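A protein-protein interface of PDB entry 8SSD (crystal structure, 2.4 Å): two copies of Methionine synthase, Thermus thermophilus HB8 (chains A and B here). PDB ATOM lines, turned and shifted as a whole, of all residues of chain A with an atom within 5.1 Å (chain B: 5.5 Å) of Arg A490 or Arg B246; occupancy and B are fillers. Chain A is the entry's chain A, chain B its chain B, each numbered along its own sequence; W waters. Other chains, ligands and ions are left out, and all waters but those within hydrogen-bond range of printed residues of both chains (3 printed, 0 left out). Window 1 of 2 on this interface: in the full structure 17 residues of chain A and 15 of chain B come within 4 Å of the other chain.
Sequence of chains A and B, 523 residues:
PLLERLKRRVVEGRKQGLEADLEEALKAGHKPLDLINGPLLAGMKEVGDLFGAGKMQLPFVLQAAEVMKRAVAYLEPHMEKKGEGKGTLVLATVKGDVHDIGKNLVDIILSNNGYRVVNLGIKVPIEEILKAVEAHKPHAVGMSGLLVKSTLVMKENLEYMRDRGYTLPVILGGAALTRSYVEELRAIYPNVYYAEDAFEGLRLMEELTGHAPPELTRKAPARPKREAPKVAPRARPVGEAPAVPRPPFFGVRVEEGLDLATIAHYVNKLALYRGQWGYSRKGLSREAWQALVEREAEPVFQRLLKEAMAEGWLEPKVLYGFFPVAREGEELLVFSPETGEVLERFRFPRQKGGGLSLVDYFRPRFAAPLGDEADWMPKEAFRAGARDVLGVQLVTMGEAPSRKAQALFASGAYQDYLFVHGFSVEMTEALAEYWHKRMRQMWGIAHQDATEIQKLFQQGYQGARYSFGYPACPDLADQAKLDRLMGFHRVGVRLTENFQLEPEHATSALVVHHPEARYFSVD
No position is printed for both chains. Of the 16 pairs that touch across the chains among the printed residues, none has its exchanged pair printed and touching as well.
Of the printed residues of chain A, Gly B444 touches His A489 and Arg A490. Of the printed residues of chain B, Leu A485 touches Arg B246. Trp B376 touches none of the printed residues of chain A. Phe A323 touches none of the printed residues of chain B. The nearest printed residue of chain B that does not touch Arg A490 is His B447 (4.2 Å). The nearest printed residue of chain A that does not touch Arg B246 is His A489 (4.7 Å). The nearest printed residue of chain B that does not touch Val A252 is Pro B247 (4.8 Å).
Among the printed residues, pairs that only touch across the chains: Gly A251 with Arg B246 (3.8 Å), Val A252 with Pro B248 (3.9 Å), Arg A253 with Pro B248 (3.5 Å), Val A254 with Met B442 (3.99 Å), Met A486 with Arg B246 (3.7 Å), His A489 with Gly B444 (3.8 Å), His A489 with His B447 (3.4 Å), Arg A490 with Arg B246 (3.3 Å), Arg A490 with Pro B248 (3.95 Å), Arg A490 with Gln B441 (3.8 Å), Arg A490 with Gly B444 (3.7 Å) and Val A491 with His B447 (3.8 Å).
Of the 14 printed residues of chain A, 10 touch a printed residue of chain B. Printed residues of chain A that touch a printed residue of chain B: Gly A251, Val A252, Arg A253, Val A254, Leu A485, Met A486, His A489, Arg A490, Val A491 and Gly A492. Hydrophobic or aromatic side chains of chain A within 4 Å of the printed part of chain B: Val A252 and Val A254. Printed residues of chain B that touch a printed residue of chain A: Arg B246, Pro B247, Pro B248, Gln B441, Met B442, Gly B444 and His B447. Hydrophobic or aromatic side chains of chain B within 4 Å of the printed part of chain A: His B447. Among the printed residues, 16 pairs touch across the chains. Among the printed residues, no Asp or Glu carboxylate lies within 4 Å of a Lys or Arg side-chain nitrogen of the other chain.
O of Val A252 sits at hydrogen-bond distance from NH2 of Arg A490, 3.1 Å away. The guanidinium group (NH1) of Arg A490 sits at hydrogen-bond distance from the backbone carbonyl oxygen (O) of Met A486.
Water W3 bridges the backbone carbonyl oxygen of Gln B441 (2.7 Å) and the backbone carbonyl oxygen of Arg A490 (2.7 Å). Water W2 lies within hydrogen-bond range of O of Val A254 and O of Pro B248. Water W1 lies within hydrogen-bond range of the guanidinium group (NH2) of Arg B246 and the backbone carbonyl oxygen (O) of Val A252.
The backbone carbonyl oxygen (O) of Leu A485 is in hydrogen-bond range of the guanidinium group (NH1) of Arg B246 (2.9 Å). O of Pro B247 is in hydrogen-bond range of NH2 of Arg A490 (3.2 Å). A ring nitrogen (NE2) of His B447 sits close to the backbone NH (N) of Gly A492 (3.2 Å). NH2 of Arg B246 sits close to N of Val A252 (3.3 Å).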
ATOM      1  N   GLY A 251       1.526  20.813   7.768  1.00  0.00           N
ATOM      2  CA  GLY A 251       1.238  21.798   8.807  1.00  0.00           C
ATOM      3  C   GLY A 251      -0.221  21.719   9.251  1.00  0.00           C
ATOM      4  O   GLY A 251      -0.890  20.736   8.937  1.00  0.00           O
ATOM      5  N   VAL A 252      -0.695  22.766   9.944  1.00  0.00           N
ATOM      6  CA  VAL A 252      -2.064  22.868  10.449  1.00  0.00           C
ATOM      7  C   VAL A 252      -2.641  24.237  10.057  1.00  0.00           C
ATOM      8  O   VAL A 252      -1.944  25.243  10.152  1.00  0.00           O
ATOM      9  CB  VAL A 252      -2.122  22.587  11.966  1.00  0.00           C
ATOM     10  CG1 VAL A 252      -3.514  22.811  12.560  1.00  0.00           C
ATOM     11  CG2 VAL A 252      -1.648  21.171  12.276  1.00  0.00           C
ATOM     12  N   ARG A 253      -3.924  24.239   9.635  1.00  0.00           N
ATOM     13  CA  ARG A 253      -4.648  25.399   9.112  1.00  0.00           C
ATOM     14  C   ARG A 253      -6.030  25.512   9.758  1.00  0.00           C
ATOM     15  O   ARG A 253      -6.502  24.545  10.360  1.00  0.00           O
ATOM     16  CB  ARG A 253      -4.801  25.265   7.592  1.00  0.00           C
ATOM     17  CG  ARG A 253      -3.471  25.416   6.867  1.00  0.00           C
ATOM     18  CD  ARG A 253      -3.626  25.589   5.379  1.00  0.00           C
ATOM     19  NE  ARG A 253      -2.337  25.783   4.716  1.00  0.00           N
ATOM     20  CZ  ARG A 253      -2.153  25.944   3.400  1.00  0.00           C
ATOM     21  NH1 ARG A 253      -3.161  25.872   2.543  1.00  0.00           N
ATOM     22  NH2 ARG A 253      -0.934  26.132   2.925  1.00  0.00           N
ATOM     23  N   VAL A 254      -6.648  26.696   9.592  1.00  0.00           N
ATOM     24  CA  VAL A 254      -7.931  27.068  10.188  1.00  0.00           C
ATOM     25  C   VAL A 254      -8.948  27.282   9.063  1.00  0.00           C
ATOM     26  O   VAL A 254      -8.607  27.908   8.055  1.00  0.00           O
ATOM     27  CB  VAL A 254      -7.792  28.316  11.088  1.00  0.00           C
ATOM     28  CG1 VAL A 254      -9.118  28.736  11.729  1.00  0.00           C
ATOM     29  CG2 VAL A 254      -6.731  28.101  12.167  1.00  0.00           C
ATOM     30  N   LEU A 319      -9.875  23.301  13.016  1.00  0.00           N
ATOM     31  CA  LEU A 319      -8.421  23.268  12.960  1.00  0.00           C
ATOM     32  C   LEU A 319      -8.017  21.914  12.370  1.00  0.00           C
ATOM     33  O   LEU A 319      -8.389  20.890  12.940  1.00  0.00           O
ATOM     34  CB  LEU A 319      -7.912  23.463  14.391  1.00  0.00           C
ATOM     35  CG  LEU A 319      -6.412  23.635  14.600  1.00  0.00           C
ATOM     36  CD1 LEU A 319      -5.904  24.940  14.003  1.00  0.00           C
ATOM     37  CD2 LEU A 319      -6.097  23.603  16.090  1.00  0.00           C
ATOM     38  N   PHE A 323       0.600  15.767   8.858  1.00  0.00           N
ATOM     39  CA  PHE A 323       1.941  15.659   9.414  1.00  0.00           C
ATOM     40  C   PHE A 323       2.664  14.487   8.757  1.00  0.00           C
ATOM     41  O   PHE A 323       2.037  13.465   8.511  1.00  0.00           O
ATOM     42  CB  PHE A 323       1.867  15.487  10.930  1.00  0.00           C
ATOM     43  CG  PHE A 323       1.589  16.768  11.669  1.00  0.00           C
ATOM     44  CD1 PHE A 323       2.629  17.661  11.921  1.00  0.00           C
ATOM     45  CD2 PHE A 323       0.312  17.086  12.121  1.00  0.00           C
ATOM     46  CE1 PHE A 323       2.403  18.834  12.634  1.00  0.00           C
ATOM     47  CE2 PHE A 323       0.086  18.258  12.841  1.00  0.00           C
ATOM     48  CZ  PHE A 323       1.130  19.135  13.086  1.00  0.00           C
ATOM     49  N   LEU A 485       0.931  19.745  18.798  1.00  0.00           N
ATOM     50  CA  LEU A 485       1.062  19.721  17.339  1.00  0.00           C
ATOM     51  C   LEU A 485       0.214  20.802  16.656  1.00  0.00           C
ATOM     52  O   LEU A 485       0.753  21.508  15.813  1.00  0.00           O
ATOM     53  CB  LEU A 485       0.710  18.319  16.821  1.00  0.00           C
ATOM     54  CG  LEU A 485       1.716  17.221  17.186  1.00  0.00           C
ATOM     55  CD1 LEU A 485       1.149  15.829  16.954  1.00  0.00           C
ATOM     56  CD2 LEU A 485       3.019  17.386  16.433  1.00  0.00           C
ATOM     57  N   MET A 486      -1.069  20.951  17.032  1.00  0.00           N
ATOM     58  CA  MET A 486      -2.045  21.765  16.311  1.00  0.00           C
ATOM     59  C   MET A 486      -2.179  23.186  16.881  1.00  0.00           C
ATOM     60  O   MET A 486      -2.260  24.147  16.111  1.00  0.00           O
ATOM     61  CB  MET A 486      -3.415  21.075  16.349  1.00  0.00           C
ATOM     62  CG  MET A 486      -3.477  19.730  15.608  1.00  0.00           C
ATOM     63  SD  MET A 486      -5.085  19.478  14.749  1.00  0.00           S
ATOM     64  CE  MET A 486      -5.844  18.198  15.731  1.00  0.00           C
ATOM     65  N   GLY A 487      -2.255  23.315  18.220  1.00  0.00           N
ATOM     66  CA  GLY A 487      -2.584  24.553  18.919  1.00  0.00           C
ATOM     67  C   GLY A 487      -4.100  24.762  19.001  1.00  0.00           C
ATOM     68  O   GLY A 487      -4.644  25.553  18.231  1.00  0.00           O
ATOM     69  N   PHE A 488      -4.758  24.062  19.951  1.00  0.00           N
ATOM     70  CA  PHE A 488      -6.208  24.062  20.127  1.00  0.00           C
ATOM     71  C   PHE A 488      -6.774  25.457  20.440  1.00  0.00           C
ATOM     72  O   PHE A 488      -7.919  25.708  20.074  1.00  0.00           O
ATOM     73  CB  PHE A 488      -6.629  23.064  21.216  1.00  0.00           C
ATOM     74  CG  PHE A 488      -6.510  21.577  20.945  1.00  0.00           C
ATOM     75  CD1 PHE A 488      -5.964  21.041  19.774  1.00  0.00           C
ATOM     76  CD2 PHE A 488      -6.967  20.677  21.908  1.00  0.00           C
ATOM     77  CE1 PHE A 488      -5.890  19.660  19.585  1.00  0.00           C
ATOM     78  CE2 PHE A 488      -6.874  19.295  21.725  1.00  0.00           C
ATOM     79  CZ  PHE A 488      -6.339  18.783  20.558  1.00  0.00           C
ATOM     80  N   HIS A 489      -6.001  26.330  21.125  1.00  0.00           N
ATOM     81  CA  HIS A 489      -6.317  27.742  21.360  1.00  0.00           C
ATOM     82  C   HIS A 489      -6.731  28.544  20.112  1.00  0.00           C
ATOM     83  O   HIS A 489      -7.525  29.471  20.238  1.00  0.00           O
ATOM     84  CB  HIS A 489      -5.131  28.450  22.037  1.00  0.00           C
ATOM     85  CG  HIS A 489      -3.907  28.549  21.179  1.00  0.00           C
ATOM     86  ND1 HIS A 489      -3.032  27.525  20.878  1.00  0.00           N
ATOM     87  CD2 HIS A 489      -3.478  29.619  20.501  1.00  0.00           C
ATOM     88  CE1 HIS A 489      -2.105  27.979  20.049  1.00  0.00           C
ATOM     89  NE2 HIS A 489      -2.348  29.252  19.820  1.00  0.00           N
ATOM     90  N   ARG A 490      -6.206  28.181  18.926  1.00  0.00           N
ATOM     91  CA  ARG A 490      -6.505  28.802  17.635  1.00  0.00           C
ATOM     92  C   ARG A 490      -7.992  28.767  17.247  1.00  0.00           C
ATOM     93  O   ARG A 490      -8.404  29.642  16.488  1.00  0.00           O
ATOM     94  CB  ARG A 490      -5.671  28.151  16.526  1.00  0.00           C
ATOM     95  CG  ARG A 490      -4.168  28.375  16.649  1.00  0.00           C
ATOM     96  CD  ARG A 490      -3.331  27.408  15.835  1.00  0.00           C
ATOM     97  NE  ARG A 490      -3.266  27.739  14.411  1.00  0.00           N
ATOM     98  CZ  ARG A 490      -2.882  26.910  13.430  1.00  0.00           C
ATOM     99  NH1 ARG A 490      -2.313  25.740  13.697  1.00  0.00           N
ATOM    100  NH2 ARG A 490      -3.013  27.295  12.166  1.00  0.00           N
ATOM    101  N   VAL A 491      -8.774  27.779  17.734  1.00  0.00           N
ATOM    102  CA  VAL A 491     -10.230  27.712  17.558  1.00  0.00           C
ATOM    103  C   VAL A 491     -10.962  27.771  18.911  1.00  0.00           C
ATOM    104  O   VAL A 491     -12.094  27.292  19.028  1.00  0.00           O
ATOM    105  CB  VAL A 491     -10.609  26.484  16.691  1.00  0.00           C
ATOM    106  CG1 VAL A 491     -10.130  26.652  15.257  1.00  0.00           C
ATOM    107  CG2 VAL A 491     -10.108  25.153  17.243  1.00  0.00           C
ATOM    108  N   GLY A 492     -10.372  28.450  19.915  1.00  0.00           N
ATOM    109  CA  GLY A 492     -10.980  28.656  21.225  1.00  0.00           C
ATOM    110  C   GLY A 492     -11.123  27.412  22.119  1.00  0.00           C
ATOM    111  O   GLY A 492     -11.857  27.498  23.103  1.00  0.00           O
ATOM    112  N   VAL B 244       3.852  33.465  21.112  1.00  0.00           N
ATOM    113  CA  VAL B 244       3.747  33.878  19.717  1.00  0.00           C
ATOM    114  C   VAL B 244       2.617  33.027  19.129  1.00  0.00           C
ATOM    115  O   VAL B 244       2.793  31.805  19.047  1.00  0.00           O
ATOM    116  CB  VAL B 244       5.073  33.691  18.944  1.00  0.00           C
ATOM    117  CG1 VAL B 244       4.982  34.253  17.530  1.00  0.00           C
ATOM    118  CG2 VAL B 244       6.268  34.298  19.677  1.00  0.00           C
ATOM    119  N   PRO B 245       1.457  33.592  18.692  1.00  0.00           N
ATOM    120  CA  PRO B 245       0.390  32.771  18.110  1.00  0.00           C
ATOM    121  C   PRO B 245       0.756  32.294  16.696  1.00  0.00           C
ATOM    122  O   PRO B 245       1.454  33.008  15.964  1.00  0.00           O
ATOM    123  CB  PRO B 245      -0.849  33.683  18.145  1.00  0.00           C
ATOM    124  CG  PRO B 245      -0.276  35.082  18.052  1.00  0.00           C
ATOM    125  CD  PRO B 245       1.096  35.022  18.703  1.00  0.00           C
ATOM    126  N   ARG B 246       0.264  31.090  16.345  1.00  0.00           N
ATOM    127  CA  ARG B 246       0.481  30.486  15.038  1.00  0.00           C
ATOM    128  C   ARG B 246      -0.521  31.114  14.063  1.00  0.00           C
ATOM    129  O   ARG B 246      -1.711  31.178  14.388  1.00  0.00           O
ATOM    130  CB  ARG B 246       0.308  28.964  15.116  1.00  0.00           C
ATOM    131  CG  ARG B 246       0.689  28.213  13.849  1.00  0.00           C
ATOM    132  CD  ARG B 246       0.854  26.734  14.146  1.00  0.00           C
ATOM    133  NE  ARG B 246       1.130  25.894  12.982  1.00  0.00           N
ATOM    134  CZ  ARG B 246       1.232  24.565  13.023  1.00  0.00           C
ATOM    135  NH1 ARG B 246       0.913  23.912  14.128  1.00  0.00           N
ATOM    136  NH2 ARG B 246       1.647  23.891  11.965  1.00  0.00           N
ATOM    137  N   PRO B 247      -0.102  31.615  12.864  1.00  0.00           N
ATOM    138  CA  PRO B 247      -1.065  32.129  11.885  1.00  0.00           C
ATOM    139  C   PRO B 247      -1.756  30.981  11.146  1.00  0.00           C
ATOM    140  O   PRO B 247      -1.278  29.842  11.215  1.00  0.00           O
ATOM    141  CB  PRO B 247      -0.189  32.978  10.944  1.00  0.00           C
ATOM    142  CG  PRO B 247       1.134  32.258  10.942  1.00  0.00           C
ATOM    143  CD  PRO B 247       1.276  31.707  12.347  1.00  0.00           C
ATOM    144  N   PRO B 248      -2.873  31.226  10.407  1.00  0.00           N
ATOM    145  CA  PRO B 248      -3.477  30.209   9.536  1.00  0.00           C
ATOM    146  C   PRO B 248      -2.545  29.689   8.439  1.00  0.00           C
ATOM    147  O   PRO B 248      -2.587  28.505   8.142  1.00  0.00           O
ATOM    148  CB  PRO B 248      -4.698  30.947   8.947  1.00  0.00           C
ATOM    149  CG  PRO B 248      -4.296  32.386   8.962  1.00  0.00           C
ATOM    150  CD  PRO B 248      -3.593  32.505  10.294  1.00  0.00           C
ATOM    151  N   TRP B 376       6.984  24.974  14.147  1.00  0.00           N
ATOM    152  CA  TRP B 376       6.047  25.450  13.117  1.00  0.00           C
ATOM    153  C   TRP B 376       6.500  26.699  12.352  1.00  0.00           C
ATOM    154  O   TRP B 376       5.968  26.907  11.263  1.00  0.00           O
ATOM    155  CB  TRP B 376       4.642  25.641  13.709  1.00  0.00           C
ATOM    156  CG  TRP B 376       4.547  26.556  14.895  1.00  0.00           C
ATOM    157  CD1 TRP B 376       4.418  26.165  16.186  1.00  0.00           C
ATOM    158  CD2 TRP B 376       4.496  27.996  14.909  1.00  0.00           C
ATOM    159  NE1 TRP B 376       4.324  27.248  17.012  1.00  0.00           N
ATOM    160  CE2 TRP B 376       4.368  28.389  16.264  1.00  0.00           C
ATOM    161  CE3 TRP B 376       4.529  29.005  13.925  1.00  0.00           C
ATOM    162  CZ2 TRP B 376       4.267  29.734  16.652  1.00  0.00           C
ATOM    163  CZ3 TRP B 376       4.467  30.337  14.315  1.00  0.00           C
ATOM    164  CH2 TRP B 376       4.321  30.697  15.665  1.00  0.00           C
ATOM    165  N   GLN B 441      -9.497  36.301  14.514  1.00  0.00           N
ATOM    166  CA  GLN B 441     -10.150  34.991  14.559  1.00  0.00           C
ATOM    167  C   GLN B 441      -9.278  33.909  13.916  1.00  0.00           C
ATOM    168  O   GLN B 441      -9.111  32.836  14.501  1.00  0.00           O
ATOM    169  CB  GLN B 441     -11.523  35.047  13.880  1.00  0.00           C
ATOM    170  CG  GLN B 441     -12.560  35.851  14.656  1.00  0.00           C
ATOM    171  CD  GLN B 441     -13.862  36.093  13.927  1.00  0.00           C
ATOM    172  OE1 GLN B 441     -14.014  35.772  12.749  1.00  0.00           O
ATOM    173  NE2 GLN B 441     -14.804  36.719  14.621  1.00  0.00           N
ATOM    174  N   MET B 442      -8.767  34.191  12.705  1.00  0.00           N
ATOM    175  CA  MET B 442      -7.787  33.355  12.022  1.00  0.00           C
ATOM    176  C   MET B 442      -6.540  33.094  12.872  1.00  0.00           C
ATOM    177  O   MET B 442      -6.047  31.965  12.874  1.00  0.00           O
ATOM    178  CB  MET B 442      -7.305  34.044  10.745  1.00  0.00           C
ATOM    179  CG  MET B 442      -8.249  34.000   9.588  1.00  0.00           C
ATOM    180  SD  MET B 442      -7.525  35.034   8.281  1.00  0.00           S
ATOM    181  CE  MET B 442      -8.972  35.989   7.848  1.00  0.00           C
ATOM    182  N   TRP B 443      -6.004  34.157  13.514  1.00  0.00           N
ATOM    183  CA  TRP B 443      -4.734  34.085  14.239  1.00  0.00           C
ATOM    184  C   TRP B 443      -4.885  33.340  15.577  1.00  0.00           C
ATOM    185  O   TRP B 443      -3.869  32.886  16.113  1.00  0.00           O
ATOM    186  CB  TRP B 443      -4.118  35.493  14.418  1.00  0.00           C
ATOM    187  CG  TRP B 443      -2.624  35.608  14.416  1.00  0.00           C
ATOM    188  CD1 TRP B 443      -1.686  34.621  14.487  1.00  0.00           C
ATOM    189  CD2 TRP B 443      -1.893  36.840  14.321  1.00  0.00           C
ATOM    190  NE1 TRP B 443      -0.425  35.143  14.429  1.00  0.00           N
ATOM    191  CE2 TRP B 443      -0.518  36.507  14.354  1.00  0.00           C
ATOM    192  CE3 TRP B 443      -2.268  38.190  14.247  1.00  0.00           C
ATOM    193  CZ2 TRP B 443       0.478  37.475  14.270  1.00  0.00           C
ATOM    194  CZ3 TRP B 443      -1.283  39.154  14.176  1.00  0.00           C
ATOM    195  CH2 TRP B 443       0.074  38.795  14.176  1.00  0.00           C
ATOM    196  N   GLY B 444      -6.115  33.234  16.128  1.00  0.00           N
ATOM    197  CA  GLY B 444      -6.371  32.582  17.400  1.00  0.00           C
ATOM    198  C   GLY B 444      -6.356  33.529  18.598  1.00  0.00           C
ATOM    199  O   GLY B 444      -6.244  33.038  19.719  1.00  0.00           O
ATOM    200  N   HIS B 447     -10.612  35.575  21.146  1.00  0.00           N
ATOM    201  CA  HIS B 447     -11.501  35.069  22.194  1.00  0.00           C
ATOM    202  C   HIS B 447     -11.695  36.061  23.354  1.00  0.00           C
ATOM    203  O   HIS B 447     -12.544  35.784  24.201  1.00  0.00           O
ATOM    204  CB  HIS B 447     -11.083  33.659  22.631  1.00  0.00           C
ATOM    205  CG  HIS B 447     -11.049  32.732  21.463  1.00  0.00           C
ATOM    206  ND1 HIS B 447      -9.858  32.389  20.865  1.00  0.00           N
ATOM    207  CD2 HIS B 447     -12.019  32.209  20.705  1.00  0.00           C
ATOM    208  CE1 HIS B 447     -10.107  31.606  19.825  1.00  0.00           C
ATOM    209  NE2 HIS B 447     -11.414  31.486  19.704  1.00  0.00           N
HETATM  210  O   HOH W   1       1.273  25.392   9.414  1.00  0.00           O
HETATM  211  O   HOH W   2      -5.895  28.494   7.149  1.00  0.00           O
HETATM  212  O   HOH W   3     -10.529  30.610  15.092  1.00  0.00           O
